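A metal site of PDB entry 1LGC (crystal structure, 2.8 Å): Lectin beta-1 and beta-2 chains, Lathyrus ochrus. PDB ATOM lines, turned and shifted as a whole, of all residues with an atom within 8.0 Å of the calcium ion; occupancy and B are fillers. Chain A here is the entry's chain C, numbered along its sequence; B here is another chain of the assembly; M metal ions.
The calcium ion is bound by the side-chain amide oxygen (OD1) of Asn 125 (1.9 Å), the side-chain carboxylate (OD1) of Asp 121 (2.3 Å), the backbone carbonyl oxygen (O) of Phe 123 (2.5 Å) and the side-chain carboxylate (OD2) of Asp 121 (2.6 Å). The calcium ion has four donor atoms within binding distance.
Asp 81 touches the calcium ion. OD2 of Asp 129 touches the calcium ion (3.5 Å). Within 4 Å of the calcium ion: Asp 81, Asp 121, Phe 123, Asn 125 and Asp 129. The nearest printed residue that does not touch the calcium ion is Gly 99 (4.2 Å).
N of Asn 125 lies within hydrogen-bond range of OD2 of Asp 129, 2.8 Å away. N of Asp 81 lies within hydrogen-bond range of O of Thr 27 of chain B, at 3.0 Å. The side-chain carboxylate of Asp 129 sits close to a ring nitrogen (NE2) of His 136 (3.1 Å). The indole nitrogen (NE1) of Trp 128 lies close to the side-chain amide oxygen (OD1) of Asn 125, 3.5 Å away. The backbone carbonyl oxygen of Asp 121 is in hydrogen-bond range of the backbone NH of His 136, 3.0 Å away.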
ATOM      1  N   VAL A  79      32.445  36.018  18.465  1.00  0.00           N
ATOM      2  CA  VAL A  79      32.511  34.584  18.669  1.00  0.00           C
ATOM      3  C   VAL A  79      31.774  33.835  17.571  1.00  0.00           C
ATOM      4  O   VAL A  79      30.785  34.316  17.031  1.00  0.00           O
ATOM      5  CB  VAL A  79      31.913  34.192  20.022  1.00  0.00           C
ATOM      6  CG1 VAL A  79      32.071  32.719  20.260  1.00  0.00           C
ATOM      7  CG2 VAL A  79      32.588  34.965  21.129  1.00  0.00           C
ATOM      8  N   ALA A  80      32.290  32.657  17.232  1.00  0.00           N
ATOM      9  CA  ALA A  80      31.716  31.773  16.212  1.00  0.00           C
ATOM     10  C   ALA A  80      32.429  30.419  16.339  1.00  0.00           C
ATOM     11  O   ALA A  80      33.537  30.356  16.903  1.00  0.00           O
ATOM     12  CB  ALA A  80      31.907  32.340  14.818  1.00  0.00           C
ATOM     13  N   ASP A  81      31.820  29.344  15.861  1.00  0.00           N
ATOM     14  CA  ASP A  81      30.516  29.367  15.198  1.00  0.00           C
ATOM     15  C   ASP A  81      29.421  28.628  15.964  1.00  0.00           C
ATOM     16  O   ASP A  81      28.232  28.793  15.651  1.00  0.00           O
ATOM     17  CB  ASP A  81      30.637  28.744  13.821  1.00  0.00           C
ATOM     18  CG  ASP A  81      30.182  29.664  12.731  1.00  0.00           C
ATOM     19  OD1 ASP A  81      28.995  30.049  12.736  1.00  0.00           O
ATOM     20  OD2 ASP A  81      31.033  29.993  11.878  1.00  0.00           O
ATOM     21  N   GLY A  82      29.814  27.827  16.941  1.00  0.00           N
ATOM     22  CA  GLY A  82      28.841  27.074  17.702  1.00  0.00           C
ATOM     23  C   GLY A  82      29.322  25.723  18.215  1.00  0.00           C
ATOM     24  O   GLY A  82      30.527  25.472  18.271  1.00  0.00           O
ATOM     25  N   GLY A  98      31.250  26.170   9.047  1.00  0.00           N
ATOM     26  CA  GLY A  98      30.847  27.529   9.331  1.00  0.00           C
ATOM     27  C   GLY A  98      29.494  27.605   9.999  1.00  0.00           C
ATOM     28  O   GLY A  98      29.223  26.918  10.992  1.00  0.00           O
ATOM     29  N   GLY A  99      28.609  28.389   9.394  1.00  0.00           N
ATOM     30  CA  GLY A  99      27.278  28.571   9.930  1.00  0.00           C
ATOM     31  C   GLY A  99      26.457  27.308  10.045  1.00  0.00           C
ATOM     32  O   GLY A  99      25.489  27.269  10.797  1.00  0.00           O
ATOM     33  N   TYR A 100      26.852  26.274   9.312  1.00  0.00           N
ATOM     34  CA  TYR A 100      26.129  25.002   9.329  1.00  0.00           C
ATOM     35  C   TYR A 100      26.603  24.045  10.410  1.00  0.00           C
ATOM     36  O   TYR A 100      26.133  22.901  10.480  1.00  0.00           O
ATOM     37  CB  TYR A 100      26.207  24.349   7.956  1.00  0.00           C
ATOM     38  CG  TYR A 100      25.551  25.133   6.857  1.00  0.00           C
ATOM     39  CD1 TYR A 100      26.227  26.156   6.204  1.00  0.00           C
ATOM     40  CD2 TYR A 100      24.259  24.850   6.449  1.00  0.00           C
ATOM     41  CE1 TYR A 100      25.641  26.868   5.182  1.00  0.00           C
ATOM     42  CE2 TYR A 100      23.665  25.555   5.425  1.00  0.00           C
ATOM     43  CZ  TYR A 100      24.359  26.569   4.788  1.00  0.00           C
ATOM     44  OH  TYR A 100      23.757  27.268   3.762  1.00  0.00           O
ATOM     45  N   LEU A 101      27.511  24.505  11.276  1.00  0.00           N
ATOM     46  CA  LEU A 101      28.056  23.685  12.354  1.00  0.00           C
ATOM     47  C   LEU A 101      28.626  22.336  11.902  1.00  0.00           C
ATOM     48  O   LEU A 101      28.759  21.406  12.692  1.00  0.00           O
ATOM     49  CB  LEU A 101      26.996  23.466  13.460  1.00  0.00           C
ATOM     50  CG  LEU A 101      26.515  24.639  14.329  1.00  0.00           C
ATOM     51  CD1 LEU A 101      27.682  25.499  14.761  1.00  0.00           C
ATOM     52  CD2 LEU A 101      25.513  25.463  13.572  1.00  0.00           C
ATOM     53  N   GLU A 119      21.774  22.423  19.186  1.00  0.00           N
ATOM     54  CA  GLU A 119      22.947  23.255  19.033  1.00  0.00           C
ATOM     55  C   GLU A 119      22.969  24.424  19.997  1.00  0.00           C
ATOM     56  O   GLU A 119      21.979  24.737  20.651  1.00  0.00           O
ATOM     57  CB  GLU A 119      23.000  23.799  17.627  1.00  0.00           C
ATOM     58  CG  GLU A 119      21.835  24.699  17.324  1.00  0.00           C
ATOM     59  CD  GLU A 119      21.938  25.310  15.965  1.00  0.00           C
ATOM     60  OE1 GLU A 119      21.641  24.611  14.976  1.00  0.00           O
ATOM     61  OE2 GLU A 119      22.350  26.493  15.889  1.00  0.00           O
ATOM     62  N   PHE A 120      24.123  25.080  20.044  1.00  0.00           N
ATOM     63  CA  PHE A 120      24.365  26.236  20.866  1.00  0.00           C
ATOM     64  C   PHE A 120      25.063  27.168  19.898  1.00  0.00           C
ATOM     65  O   PHE A 120      26.279  27.202  19.842  1.00  0.00           O
ATOM     66  CB  PHE A 120      25.281  25.854  22.014  1.00  0.00           C
ATOM     67  CG  PHE A 120      24.773  24.700  22.823  1.00  0.00           C
ATOM     68  CD1 PHE A 120      25.065  23.396  22.471  1.00  0.00           C
ATOM     69  CD2 PHE A 120      24.020  24.924  23.968  1.00  0.00           C
ATOM     70  CE1 PHE A 120      24.606  22.305  23.236  1.00  0.00           C
ATOM     71  CE2 PHE A 120      23.557  23.865  24.748  1.00  0.00           C
ATOM     72  CZ  PHE A 120      23.854  22.542  24.386  1.00  0.00           C
ATOM     73  N   ASP A 121      24.275  27.829  19.052  1.00  0.00           N
ATOM     74  CA  ASP A 121      24.800  28.742  18.036  1.00  0.00           C
ATOM     75  C   ASP A 121      25.279  30.031  18.682  1.00  0.00           C
ATOM     76  O   ASP A 121      24.508  30.723  19.357  1.00  0.00           O
ATOM     77  CB  ASP A 121      23.722  29.049  16.991  1.00  0.00           C
ATOM     78  CG  ASP A 121      24.284  29.695  15.719  1.00  0.00           C
ATOM     79  OD1 ASP A 121      25.479  30.084  15.711  1.00  0.00           O
ATOM     80  OD2 ASP A 121      23.530  29.810  14.732  1.00  0.00           O
ATOM     81  N   THR A 122      26.535  30.372  18.429  1.00  0.00           N
ATOM     82  CA  THR A 122      27.162  31.565  18.972  1.00  0.00           C
ATOM     83  C   THR A 122      27.404  32.643  17.933  1.00  0.00           C
ATOM     84  O   THR A 122      28.202  33.538  18.162  1.00  0.00           O
ATOM     85  CB  THR A 122      28.521  31.225  19.586  1.00  0.00           C
ATOM     86  OG1 THR A 122      29.273  30.423  18.661  1.00  0.00           O
ATOM     87  CG2 THR A 122      28.369  30.493  20.908  1.00  0.00           C
ATOM     88  N   PHE A 123      26.711  32.574  16.794  1.00  0.00           N
ATOM     89  CA  PHE A 123      26.922  33.566  15.742  1.00  0.00           C
ATOM     90  C   PHE A 123      25.662  33.682  14.904  1.00  0.00           C
ATOM     91  O   PHE A 123      25.078  32.654  14.489  1.00  0.00           O
ATOM     92  CB  PHE A 123      28.116  33.136  14.888  1.00  0.00           C
ATOM     93  CG  PHE A 123      28.459  34.102  13.770  1.00  0.00           C
ATOM     94  CD1 PHE A 123      29.333  35.148  13.980  1.00  0.00           C
ATOM     95  CD2 PHE A 123      27.952  33.902  12.493  1.00  0.00           C
ATOM     96  CE1 PHE A 123      29.695  35.993  12.935  1.00  0.00           C
ATOM     97  CE2 PHE A 123      28.305  34.745  11.438  1.00  0.00           C
ATOM     98  CZ  PHE A 123      29.175  35.789  11.670  1.00  0.00           C
ATOM     99  N   TYR A 124      25.281  34.929  14.617  1.00  0.00           N
ATOM    100  CA  TYR A 124      24.077  35.254  13.858  1.00  0.00           C
ATOM    101  C   TYR A 124      24.206  35.066  12.350  1.00  0.00           C
ATOM    102  O   TYR A 124      24.953  35.773  11.693  1.00  0.00           O
ATOM    103  CB  TYR A 124      23.634  36.703  14.158  1.00  0.00           C
ATOM    104  CG  TYR A 124      22.402  37.149  13.360  1.00  0.00           C
ATOM    105  CD1 TYR A 124      21.202  36.469  13.476  1.00  0.00           C
ATOM    106  CD2 TYR A 124      22.479  38.210  12.452  1.00  0.00           C
ATOM    107  CE1 TYR A 124      20.114  36.815  12.720  1.00  0.00           C
ATOM    108  CE2 TYR A 124      21.388  38.565  11.678  1.00  0.00           C
ATOM    109  CZ  TYR A 124      20.205  37.859  11.813  1.00  0.00           C
ATOM    110  OH  TYR A 124      19.113  38.167  11.039  1.00  0.00           O
ATOM    111  N   ASN A 125      23.428  34.144  11.804  1.00  0.00           N
ATOM    112  CA  ASN A 125      23.417  33.881  10.362  1.00  0.00           C
ATOM    113  C   ASN A 125      22.021  34.227   9.878  1.00  0.00           C
ATOM    114  O   ASN A 125      21.044  33.495  10.136  1.00  0.00           O
ATOM    115  CB  ASN A 125      23.737  32.422  10.055  1.00  0.00           C
ATOM    116  CG  ASN A 125      25.013  31.943  10.729  1.00  0.00           C
ATOM    117  OD1 ASN A 125      24.951  31.330  11.813  1.00  0.00           O
ATOM    118  ND2 ASN A 125      26.167  32.210  10.111  1.00  0.00           N
ATOM    119  N   THR A 126      21.935  35.365   9.201  1.00  0.00           N
ATOM    120  CA  THR A 126      20.699  35.939   8.688  1.00  0.00           C
ATOM    121  C   THR A 126      19.578  35.045   8.187  1.00  0.00           C
ATOM    122  O   THR A 126      18.534  34.958   8.818  1.00  0.00           O
ATOM    123  CB  THR A 126      20.992  36.969   7.608  1.00  0.00           C
ATOM    124  OG1 THR A 126      22.212  37.657   7.928  1.00  0.00           O
ATOM    125  CG2 THR A 126      19.859  37.983   7.544  1.00  0.00           C
ATOM    126  N   TRP A 128      18.673  32.162   8.510  1.00  0.00           N
ATOM    127  CA  TRP A 128      18.265  30.997   9.276  1.00  0.00           C
ATOM    128  C   TRP A 128      18.289  31.161  10.793  1.00  0.00           C
ATOM    129  O   TRP A 128      17.763  30.311  11.537  1.00  0.00           O
ATOM    130  CB  TRP A 128      19.010  29.730   8.802  1.00  0.00           C
ATOM    131  CG  TRP A 128      20.510  29.706   8.996  1.00  0.00           C
ATOM    132  CD1 TRP A 128      21.189  29.653  10.182  1.00  0.00           C
ATOM    133  CD2 TRP A 128      21.505  29.697   7.971  1.00  0.00           C
ATOM    134  NE1 TRP A 128      22.535  29.615   9.958  1.00  0.00           N
ATOM    135  CE2 TRP A 128      22.768  29.634   8.610  1.00  0.00           C
ATOM    136  CE3 TRP A 128      21.465  29.736   6.575  1.00  0.00           C
ATOM    137  CZ2 TRP A 128      23.972  29.618   7.905  1.00  0.00           C
ATOM    138  CZ3 TRP A 128      22.668  29.706   5.865  1.00  0.00           C
ATOM    139  CH2 TRP A 128      23.901  29.654   6.536  1.00  0.00           C
ATOM    140  N   ASP A 129      18.892  32.243  11.275  1.00  0.00           N
ATOM    141  CA  ASP A 129      18.916  32.493  12.709  1.00  0.00           C
ATOM    142  C   ASP A 129      17.880  33.567  13.072  1.00  0.00           C
ATOM    143  O   ASP A 129      17.539  34.407  12.239  1.00  0.00           O
ATOM    144  CB  ASP A 129      20.315  32.887  13.163  1.00  0.00           C
ATOM    145  CG  ASP A 129      21.232  31.684  13.351  1.00  0.00           C
ATOM    146  OD1 ASP A 129      20.799  30.685  13.965  1.00  0.00           O
ATOM    147  OD2 ASP A 129      22.408  31.750  12.913  1.00  0.00           O
ATOM    148  N   HIS A 136      22.043  31.317  20.897  1.00  0.00           N
ATOM    149  CA  HIS A 136      20.946  30.505  21.382  1.00  0.00           C
ATOM    150  C   HIS A 136      21.036  28.999  21.246  1.00  0.00           C
ATOM    151  O   HIS A 136      21.667  28.478  20.327  1.00  0.00           O
ATOM    152  CB  HIS A 136      19.710  30.920  20.603  1.00  0.00           C
ATOM    153  CG  HIS A 136      19.930  30.898  19.126  1.00  0.00           C
ATOM    154  ND1 HIS A 136      20.760  31.782  18.494  1.00  0.00           N
ATOM    155  CD2 HIS A 136      19.459  30.064  18.169  1.00  0.00           C
ATOM    156  CE1 HIS A 136      20.796  31.513  17.210  1.00  0.00           C
ATOM    157  NE2 HIS A 136      20.018  30.471  16.975  1.00  0.00           N
ATOM    158  N   ILE A 144      19.606  23.631   9.047  1.00  0.00           N
ATOM    159  CA  ILE A 144      20.275  24.520   9.987  1.00  0.00           C
ATOM    160  C   ILE A 144      19.314  25.550  10.585  1.00  0.00           C
ATOM    161  O   ILE A 144      19.621  26.218  11.591  1.00  0.00           O
ATOM    162  CB  ILE A 144      21.466  25.256   9.328  1.00  0.00           C
ATOM    163  CG1 ILE A 144      22.333  25.960  10.383  1.00  0.00           C
ATOM    164  CG2 ILE A 144      20.956  26.279   8.329  1.00  0.00           C
ATOM    165  CD1 ILE A 144      22.973  25.035  11.385  1.00  0.00           C
ATOM    166  N   THR B  27      32.432  24.270  14.912  1.00  0.00           N
ATOM    167  CA  THR B  27      33.059  24.859  13.737  1.00  0.00           C
ATOM    168  C   THR B  27      33.424  26.302  13.982  1.00  0.00           C
ATOM    169  O   THR B  27      33.183  26.839  15.058  1.00  0.00           O
ATOM    170  CB  THR B  27      32.099  24.884  12.539  1.00  0.00           C
ATOM    171  OG1 THR B  27      30.946  25.647  12.885  1.00  0.00           O
ATOM    172  CG2 THR B  27      31.697  23.476  12.104  1.00  0.00           C
HETATM  173 CA    CA M   1      25.676  30.522  13.427  1.00  0.00          CA
HETATM  174 MN    MN M   2      20.455  28.423  14.693  1.00  0.00          MN
